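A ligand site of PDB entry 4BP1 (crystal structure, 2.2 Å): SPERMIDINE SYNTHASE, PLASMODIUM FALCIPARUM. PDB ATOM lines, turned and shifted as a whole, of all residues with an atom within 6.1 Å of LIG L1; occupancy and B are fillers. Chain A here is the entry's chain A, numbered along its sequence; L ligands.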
ATOM      1  N   GLN A  34      10.816 -13.334  29.943  1.00  0.00           N
ATOM      2  CA  GLN A  34       9.409 -13.135  30.186  1.00  0.00           C
ATOM      3  C   GLN A  34       8.731 -14.204  31.043  1.00  0.00           C
ATOM      4  O   GLN A  34       9.323 -15.248  31.292  1.00  0.00           O
ATOM      5  CB  GLN A  34       8.669 -12.879  28.829  1.00  0.00           C
ATOM      6  CG  GLN A  34       8.846 -13.932  27.776  1.00  0.00           C
ATOM      7  CD  GLN A  34       8.737 -13.487  26.278  1.00  0.00           C
ATOM      8  OE1 GLN A  34       8.161 -12.449  25.898  1.00  0.00           O
ATOM      9  NE2 GLN A  34       9.298 -14.329  25.430  1.00  0.00           N
ATOM     10  N   LEU A  48      -0.673 -20.673  24.810  1.00  0.00           N
ATOM     11  CA  LEU A  48       0.639 -20.264  25.186  1.00  0.00           C
ATOM     12  C   LEU A  48       0.495 -18.815  25.505  1.00  0.00           C
ATOM     13  O   LEU A  48      -0.015 -18.049  24.668  1.00  0.00           O
ATOM     14  CB  LEU A  48       1.611 -20.452  24.054  1.00  0.00           C
ATOM     15  CG  LEU A  48       3.006 -19.761  24.200  1.00  0.00           C
ATOM     16  CD1 LEU A  48       3.749 -20.459  25.322  1.00  0.00           C
ATOM     17  CD2 LEU A  48       3.890 -19.827  22.966  1.00  0.00           C
ATOM     18  N   LEU A  50       2.520 -15.330  27.203  1.00  0.00           N
ATOM     19  CA  LEU A  50       3.754 -14.637  27.585  1.00  0.00           C
ATOM     20  C   LEU A  50       3.438 -13.302  28.178  1.00  0.00           C
ATOM     21  O   LEU A  50       2.700 -12.559  27.553  1.00  0.00           O
ATOM     22  CB  LEU A  50       4.661 -14.430  26.369  1.00  0.00           C
ATOM     23  CG  LEU A  50       5.167 -15.692  25.629  1.00  0.00           C
ATOM     24  CD1 LEU A  50       5.980 -15.331  24.395  1.00  0.00           C
ATOM     25  CD2 LEU A  50       6.038 -16.577  26.516  1.00  0.00           C
ATOM     26  N   GLN A  55      -0.398 -15.644  23.062  1.00  0.00           N
ATOM     27  CA  GLN A  55       0.399 -15.638  21.833  1.00  0.00           C
ATOM     28  C   GLN A  55      -0.274 -16.536  20.797  1.00  0.00           C
ATOM     29  O   GLN A  55      -0.250 -16.259  19.608  1.00  0.00           O
ATOM     30  CB  GLN A  55       1.806 -16.169  22.100  1.00  0.00           C
ATOM     31  CG  GLN A  55       2.519 -15.393  23.186  1.00  0.00           C
ATOM     32  CD  GLN A  55       2.647 -13.951  22.809  1.00  0.00           C
ATOM     33  OE1 GLN A  55       2.205 -13.025  23.539  1.00  0.00           O
ATOM     34  NE2 GLN A  55       3.219 -13.733  21.654  1.00  0.00           N
ATOM     35  N   LEU A  56      -0.770 -17.648  21.244  1.00  0.00           N
ATOM     36  CA  LEU A  56      -1.513 -18.505  20.340  1.00  0.00           C
ATOM     37  C   LEU A  56      -2.345 -19.498  21.089  1.00  0.00           C
ATOM     38  O   LEU A  56      -2.079 -19.754  22.259  1.00  0.00           O
ATOM     39  CB  LEU A  56      -0.543 -19.314  19.468  1.00  0.00           C
ATOM     40  CG  LEU A  56       0.375 -20.291  20.198  1.00  0.00           C
ATOM     41  CD1 LEU A  56      -0.189 -21.690  20.302  1.00  0.00           C
ATOM     42  CD2 LEU A  56       1.649 -20.306  19.374  1.00  0.00           C
ATOM     43  N   VAL A  85      11.495 -13.422  12.372  1.00  0.00           N
ATOM     44  CA  VAL A  85      11.789 -12.781  13.692  1.00  0.00           C
ATOM     45  C   VAL A  85      10.686 -13.170  14.703  1.00  0.00           C
ATOM     46  O   VAL A  85       9.493 -13.168  14.381  1.00  0.00           O
ATOM     47  CB  VAL A  85      11.859 -11.269  13.582  1.00  0.00           C
ATOM     48  CG1 VAL A  85      11.998 -10.619  14.958  1.00  0.00           C
ATOM     49  CG2 VAL A  85      12.976 -10.855  12.635  1.00  0.00           C
ATOM     50  N   GLY A  86      11.088 -13.509  15.939  1.00  0.00           N
ATOM     51  CA  GLY A  86      10.151 -14.028  16.902  1.00  0.00           C
ATOM     52  C   GLY A  86       9.710 -15.414  16.469  1.00  0.00           C
ATOM     53  O   GLY A  86      10.517 -16.190  16.028  1.00  0.00           O
ATOM     54  N   GLY A  87       8.436 -15.717  16.607  1.00  0.00           N
ATOM     55  CA  GLY A  87       7.864 -16.969  16.113  1.00  0.00           C
ATOM     56  C   GLY A  87       8.435 -18.260  16.699  1.00  0.00           C
ATOM     57  O   GLY A  87       8.342 -19.311  16.079  1.00  0.00           O
ATOM     58  N   GLY A  88       8.957 -18.173  17.931  1.00  0.00           N
ATOM     59  CA  GLY A  88       9.578 -19.296  18.616  1.00  0.00           C
ATOM     60  C   GLY A  88       8.739 -20.541  18.716  1.00  0.00           C
ATOM     61  O   GLY A  88       9.250 -21.635  18.867  1.00  0.00           O
ATOM     62  N   ASP A  89       7.427 -20.376  18.678  1.00  0.00           N
ATOM     63  CA  ASP A  89       6.529 -21.498  18.698  1.00  0.00           C
ATOM     64  C   ASP A  89       6.703 -22.333  17.466  1.00  0.00           C
ATOM     65  O   ASP A  89       6.326 -23.531  17.456  1.00  0.00           O
ATOM     66  CB  ASP A  89       5.042 -21.018  18.766  1.00  0.00           C
ATOM     67  CG  ASP A  89       4.701 -20.009  17.667  1.00  0.00           C
ATOM     68  OD1 ASP A  89       4.978 -18.798  17.856  1.00  0.00           O
ATOM     69  OD2 ASP A  89       4.236 -20.448  16.593  1.00  0.00           O
ATOM     70  N   CYS A 108      15.235 -15.993  14.166  1.00  0.00           N
ATOM     71  CA  CYS A 108      15.948 -15.316  15.232  1.00  0.00           C
ATOM     72  C   CYS A 108      14.916 -15.021  16.342  1.00  0.00           C
ATOM     73  O   CYS A 108      14.040 -14.192  16.153  1.00  0.00           O
ATOM     74  CB  CYS A 108      16.564 -14.064  14.713  1.00  0.00           C
ATOM     75  SG  CYS A 108      17.387 -13.053  15.986  1.00  0.00           S
ATOM     76  N   GLU A 109      14.981 -15.775  17.446  1.00  0.00           N
ATOM     77  CA  GLU A 109      14.107 -15.681  18.613  1.00  0.00           C
ATOM     78  C   GLU A 109      14.950 -15.381  19.847  1.00  0.00           C
ATOM     79  O   GLU A 109      15.985 -16.009  20.112  1.00  0.00           O
ATOM     80  CB  GLU A 109      13.361 -16.995  18.790  1.00  0.00           C
ATOM     81  CG  GLU A 109      12.801 -17.322  20.156  1.00  0.00           C
ATOM     82  CD  GLU A 109      11.562 -16.521  20.505  1.00  0.00           C
ATOM     83  OE1 GLU A 109      10.548 -16.622  19.757  1.00  0.00           O
ATOM     84  OE2 GLU A 109      11.617 -15.763  21.506  1.00  0.00           O
ATOM     85  N   ILE A 110      14.511 -14.420  20.641  1.00  0.00           N
ATOM     86  CA  ILE A 110      15.284 -13.964  21.757  1.00  0.00           C
ATOM     87  C   ILE A 110      15.252 -14.986  22.912  1.00  0.00           C
ATOM     88  O   ILE A 110      16.232 -15.160  23.652  1.00  0.00           O
ATOM     89  CB  ILE A 110      14.792 -12.601  22.187  1.00  0.00           C
ATOM     90  CG1 ILE A 110      15.817 -11.947  23.080  1.00  0.00           C
ATOM     91  CG2 ILE A 110      13.408 -12.720  22.832  1.00  0.00           C
ATOM     92  CD1 ILE A 110      15.531 -10.480  23.386  1.00  0.00           C
ATOM     93  N   ASP A 111      14.174 -15.740  23.013  1.00  0.00           N
ATOM     94  CA  ASP A 111      13.910 -16.567  24.209  1.00  0.00           C
ATOM     95  C   ASP A 111      13.855 -18.060  23.930  1.00  0.00           C
ATOM     96  O   ASP A 111      12.795 -18.587  23.580  1.00  0.00           O
ATOM     97  CB  ASP A 111      12.563 -16.125  24.831  1.00  0.00           C
ATOM     98  CG  ASP A 111      12.395 -16.592  26.277  1.00  0.00           C
ATOM     99  OD1 ASP A 111      13.101 -17.531  26.701  1.00  0.00           O
ATOM    100  OD2 ASP A 111      11.507 -16.041  26.975  1.00  0.00           O
ATOM    101  N   VAL A 114      10.904 -20.426  24.884  1.00  0.00           N
ATOM    102  CA  VAL A 114       9.707 -20.479  24.074  1.00  0.00           C
ATOM    103  C   VAL A 114       9.812 -21.636  23.079  1.00  0.00           C
ATOM    104  O   VAL A 114       8.889 -22.420  22.920  1.00  0.00           O
ATOM    105  CB  VAL A 114       9.444 -19.171  23.309  1.00  0.00           C
ATOM    106  CG1 VAL A 114       8.229 -19.321  22.439  1.00  0.00           C
ATOM    107  CG2 VAL A 114       9.190 -18.015  24.259  1.00  0.00           C
ATOM    108  N   GLU A 139      18.728 -14.593  20.012  1.00  0.00           N
ATOM    109  CA  GLU A 139      19.271 -13.224  19.984  1.00  0.00           C
ATOM    110  C   GLU A 139      18.154 -12.199  19.816  1.00  0.00           C
ATOM    111  O   GLU A 139      17.151 -12.487  19.231  1.00  0.00           O
ATOM    112  CB  GLU A 139      20.193 -13.067  18.784  1.00  0.00           C
ATOM    113  CG  GLU A 139      21.452 -12.284  19.095  1.00  0.00           C
ATOM    114  CD  GLU A 139      22.384 -12.125  17.875  1.00  0.00           C
ATOM    115  OE1 GLU A 139      22.480 -13.042  17.004  1.00  0.00           O
ATOM    116  OE2 GLU A 139      23.016 -11.037  17.823  1.00  0.00           O
ATOM    117  N   ASP A 140      18.339 -11.020  20.351  1.00  0.00           N
ATOM    118  CA  ASP A 140      17.492  -9.915  20.039  1.00  0.00           C
ATOM    119  C   ASP A 140      17.607  -9.687  18.507  1.00  0.00           C
ATOM    120  O   ASP A 140      18.649  -9.223  18.025  1.00  0.00           O
ATOM    121  CB  ASP A 140      17.943  -8.682  20.819  1.00  0.00           C
ATOM    122  CG  ASP A 140      16.916  -7.498  20.770  1.00  0.00           C
ATOM    123  OD1 ASP A 140      16.282  -7.231  19.730  1.00  0.00           O
ATOM    124  OD2 ASP A 140      16.736  -6.826  21.796  1.00  0.00           O
ATOM    125  N   ALA A 141      16.533  -9.996  17.757  1.00  0.00           N
ATOM    126  CA  ALA A 141      16.467  -9.704  16.315  1.00  0.00           C
ATOM    127  C   ALA A 141      17.011  -8.303  15.959  1.00  0.00           C
ATOM    128  O   ALA A 141      17.497  -8.072  14.892  1.00  0.00           O
ATOM    129  CB  ALA A 141      15.048  -9.802  15.855  1.00  0.00           C
ATOM    130  N   SER A 142      16.882  -7.384  16.880  1.00  0.00           N
ATOM    131  CA  SER A 142      17.357  -6.055  16.675  1.00  0.00           C
ATOM    132  C   SER A 142      18.877  -5.995  16.491  1.00  0.00           C
ATOM    133  O   SER A 142      19.369  -5.204  15.690  1.00  0.00           O
ATOM    134  CB  SER A 142      16.955  -5.239  17.867  1.00  0.00           C
ATOM    135  OG  SER A 142      17.429  -3.948  17.739  1.00  0.00           O
ATOM    136  N   ASP A 158       7.092 -12.050  13.465  1.00  0.00           N
ATOM    137  CA  ASP A 158       6.040 -12.593  14.351  1.00  0.00           C
ATOM    138  C   ASP A 158       6.402 -12.300  15.789  1.00  0.00           C
ATOM    139  O   ASP A 158       6.810 -13.194  16.489  1.00  0.00           O
ATOM    140  CB  ASP A 158       5.892 -14.093  14.148  1.00  0.00           C
ATOM    141  CG  ASP A 158       4.875 -14.696  15.059  1.00  0.00           C
ATOM    142  OD1 ASP A 158       4.198 -13.932  15.755  1.00  0.00           O
ATOM    143  OD2 ASP A 158       4.733 -15.944  15.082  1.00  0.00           O
ATOM    144  N   SER A 159       6.365 -11.038  16.174  1.00  0.00           N
ATOM    145  CA  SER A 159       6.656 -10.602  17.524  1.00  0.00           C
ATOM    146  C   SER A 159       5.502 -10.737  18.467  1.00  0.00           C
ATOM    147  O   SER A 159       4.334 -10.970  18.093  1.00  0.00           O
ATOM    148  CB  SER A 159       7.016  -9.111  17.512  1.00  0.00           C
ATOM    149  OG  SER A 159       5.941  -8.336  16.928  1.00  0.00           O
ATOM    150  N   SER A 160       5.872 -10.648  19.725  1.00  0.00           N
ATOM    151  CA  SER A 160       4.931 -10.339  20.789  1.00  0.00           C
ATOM    152  C   SER A 160       4.664  -8.809  20.770  1.00  0.00           C
ATOM    153  O   SER A 160       5.148  -8.110  19.870  1.00  0.00           O
ATOM    154  CB  SER A 160       5.515 -10.841  22.117  1.00  0.00           C
ATOM    155  OG  SER A 160       6.816 -10.335  22.311  1.00  0.00           O
ATOM    156  N   GLY A 164       7.519  -5.651  26.768  1.00  0.00           N
ATOM    157  CA  GLY A 164       8.320  -6.872  26.765  1.00  0.00           C
ATOM    158  C   GLY A 164       9.571  -6.724  25.887  1.00  0.00           C
ATOM    159  O   GLY A 164       9.915  -5.619  25.464  1.00  0.00           O
ATOM    160  N   PRO A 165      10.244  -7.841  25.608  1.00  0.00           N
ATOM    161  CA  PRO A 165      11.388  -7.819  24.674  1.00  0.00           C
ATOM    162  C   PRO A 165      11.049  -7.302  23.235  1.00  0.00           C
ATOM    163  O   PRO A 165      11.930  -6.755  22.555  1.00  0.00           O
ATOM    164  CB  PRO A 165      11.852  -9.285  24.656  1.00  0.00           C
ATOM    165  CG  PRO A 165      10.642 -10.074  25.090  1.00  0.00           C
ATOM    166  CD  PRO A 165       9.914  -9.209  26.056  1.00  0.00           C
ATOM    167  N   ALA A 166       9.803  -7.425  22.789  1.00  0.00           N
ATOM    168  CA  ALA A 166       9.450  -6.919  21.450  1.00  0.00           C
ATOM    169  C   ALA A 166       9.517  -5.380  21.362  1.00  0.00           C
ATOM    170  O   ALA A 166       9.510  -4.825  20.291  1.00  0.00           O
ATOM    171  CB  ALA A 166       8.118  -7.481  20.957  1.00  0.00           C
ATOM    172  N   GLU A 167       9.646  -4.716  22.478  1.00  0.00           N
ATOM    173  CA  GLU A 167       9.934  -3.249  22.541  1.00  0.00           C
ATOM    174  C   GLU A 167      10.863  -2.687  21.432  1.00  0.00           C
ATOM    175  O   GLU A 167      10.542  -1.680  20.796  1.00  0.00           O
ATOM    176  CB  GLU A 167      10.545  -2.994  23.894  1.00  0.00           C
ATOM    177  CG  GLU A 167      10.784  -1.559  24.245  1.00  0.00           C
ATOM    178  CD  GLU A 167      11.336  -1.456  25.651  1.00  0.00           C
ATOM    179  OE1 GLU A 167      11.992  -2.425  26.131  1.00  0.00           O
ATOM    180  OE2 GLU A 167      11.088  -0.408  26.259  1.00  0.00           O
ATOM    181  N   THR A 168      11.957  -3.379  21.159  1.00  0.00           N
ATOM    182  CA  THR A 168      12.960  -2.926  20.212  1.00  0.00           C
ATOM    183  C   THR A 168      12.540  -3.134  18.770  1.00  0.00           C
ATOM    184  O   THR A 168      13.195  -2.638  17.856  1.00  0.00           O
ATOM    185  CB  THR A 168      14.312  -3.689  20.424  1.00  0.00           C
ATOM    186  OG1 THR A 168      14.102  -5.123  20.316  1.00  0.00           O
ATOM    187  CG2 THR A 168      14.906  -3.363  21.763  1.00  0.00           C
ATOM    188  N   LEU A 169      11.497  -3.893  18.539  1.00  0.00           N
ATOM    189  CA  LEU A 169      11.014  -4.126  17.193  1.00  0.00           C
ATOM    190  C   LEU A 169       9.975  -3.109  16.645  1.00  0.00           C
ATOM    191  O   LEU A 169       9.449  -3.309  15.542  1.00  0.00           O
ATOM    192  CB  LEU A 169      10.407  -5.499  17.077  1.00  0.00           C
ATOM    193  CG  LEU A 169      11.207  -6.595  17.771  1.00  0.00           C
ATOM    194  CD1 LEU A 169      10.497  -7.924  17.626  1.00  0.00           C
ATOM    195  CD2 LEU A 169      12.635  -6.686  17.267  1.00  0.00           C
HETATM  196  C1  LIG L   1       5.319 -16.530  20.273  1.00  0.00           C
HETATM  197  S1  LIG L   1       5.670 -15.497  18.908  1.00  0.00           S
HETATM  198  C2  LIG L   1       6.348 -14.058  19.566  1.00  0.00           C
HETATM  199  C3  LIG L   1       7.824 -14.283  19.885  1.00  0.00           C
HETATM  200  O1  LIG L   1       8.523 -13.029  19.751  1.00  0.00           O
HETATM  201  C4  LIG L   1       8.993 -13.650  21.887  1.00  0.00           C
HETATM  202  O2  LIG L   1       9.954 -14.115  22.809  1.00  0.00           O
HETATM  203  C5  LIG L   1       8.072 -14.700  21.340  1.00  0.00           C
HETATM  204  O3  LIG L   1       8.694 -15.929  21.341  1.00  0.00           O
HETATM  205  C6  LIG L   1       9.629 -13.200  20.596  1.00  0.00           C
HETATM  206  N1  LIG L   1      10.306 -11.922  20.714  1.00  0.00           N
HETATM  207  C7  LIG L   1       9.919 -10.837  21.421  1.00  0.00           C
HETATM  208  N2  LIG L   1      10.784  -9.839  21.288  1.00  0.00           N
HETATM  209  C8  LIG L   1      11.761 -10.330  20.478  1.00  0.00           C
HETATM  210  C9  LIG L   1      12.983  -9.811  19.917  1.00  0.00           C
HETATM  211  N3  LIG L   1      13.411  -8.543  20.197  1.00  0.00           N
HETATM  212  N4  LIG L   1      13.660 -10.636  19.115  1.00  0.00           N
HETATM  213  C10 LIG L   1      13.300 -11.874  18.809  1.00  0.00           C
HETATM  214  N5  LIG L   1      12.167 -12.436  19.269  1.00  0.00           N
HETATM  215  C11 LIG L   1      11.406 -11.693  20.100  1.00  0.00           C
HETATM  216  N1  LG2 L   2       2.221 -14.181  18.308  1.00  0.00           N
HETATM  217  C1  LG2 L   2       1.676 -12.813  18.103  1.00  0.00           C
HETATM  218  C2  LG2 L   2       1.154 -12.162  19.406  1.00  0.00           C
HETATM  219  C3  LG2 L   2       0.012 -11.115  19.300  1.00  0.00           C
HETATM  220  C4  LG2 L   2      -0.656 -10.961  20.690  1.00  0.00           C
HETATM  221  N2  LG2 L   2      -1.381  -9.706  20.950  1.00  0.00           N
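The side-chain carboxylate (OE2) of Glu 109 is in hydrogen-bond range of the backbone NH (N) of Asp 111 (3.0 Å).
N of Glu 139 lies within hydrogen-bond range of O of Glu 109 (3.1 Å).
OE1 of Glu 109 is in hydrogen-bond range of N of Gly 88, 2.9 Å away.
NE2 of Gln 34 lies within hydrogen-bond range of OD2 of Asp 111, at 3.2 Å.
OD1 of Asp 140 sits at hydrogen-bond distance from OG1 of Thr 168, 3.1 Å away.
N of Asp 158 lies within hydrogen-bond range of O of Val 85 (2.8 Å).
The backbone NH (N) of Ala 141 sits close to the side-chain sulfur (SG) of Cys 108.
The side-chain sulfur (SG) of Cys 108 sits at hydrogen-bond distance from the backbone carbonyl oxygen (O) of Glu 139.
O3 of LIG L1 lies within hydrogen-bond range of OE1 of Glu 109 (2.5 Å).
An oxygen (O2) of LIG L1 sits at hydrogen-bond distance from the side-chain amide nitrogen of Gln 34, at 2.7 Å.
N of Ala 166 sits at hydrogen-bond distance from N2 of LIG L1 (3.0 Å).
The side-chain carboxylate (OD1) of Asp 140 lies within hydrogen-bond range of a nitrogen (N3) of LIG L1, at 3.2 Å.
The backbone carbonyl oxygen (O) of Pro 165 is in hydrogen-bond range of a nitrogen (N3) of LIG L1.
A nitrogen (N4) of LIG L1 lies within hydrogen-bond range of the backbone NH of Ala 141, at 3.2 Å.
The backbone NH of Ile 110 sits close to a nitrogen (N5) of LIG L1 (3.4 Å).
OG1 of Thr 168 lies within hydrogen-bond range of N3 of LIG L1, 3.5 Å away.
The backbone NH (N) of Gly 87 sits close to a sulfur (S1) of LIG L1 (3.6 Å).
N1 of LG2 L2 is in salt-bridge range of OD1 of Asp 158 (3.2 Å).
The backbone carbonyl oxygen (O) of Gln 55 lies within hydrogen-bond range of a nitrogen (N1) of LG2 L2 (3.5 Å).
S1 of LIG L1 lies close to N1 of LG2 L2 (3.7 Å).
The side-chain carboxylate of Asp 89 lies close to a sulfur (S1) of LIG L1 (3.5 Å).
A sulfur (S1) of LIG L1 sits close to the backbone carbonyl oxygen (O) of Asp 158, at 3.5 Å.
Merely in contact with LIG L1: Ser 160, Gly 86, Leu 169, Val 114, Ser 159, Cys 108, Leu 50, Gln 55, Asp 111 and Glu 139.
Hydrophobic or aromatic side chains that line LIG L1: Leu 50, Ile 110, Val 114, Ala 141, Pro 165, Ala 166 and Leu 169.
Within 4 Å of LIG L1: Gln 34, Leu 50, Gln 55, Gly 86, Gly 87, Asp 89, Cys 108, Glu 109, Ile 110, Asp 111, Val 114, Glu 139, Asp 140, Ala 141, Asp 158, Ser 159, Ser 160, Pro 165, Ala 166, Thr 168 and Leu 169.
The nearest printed residue that does not touch LIG L1 is Gly 88 (4.1 Å).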
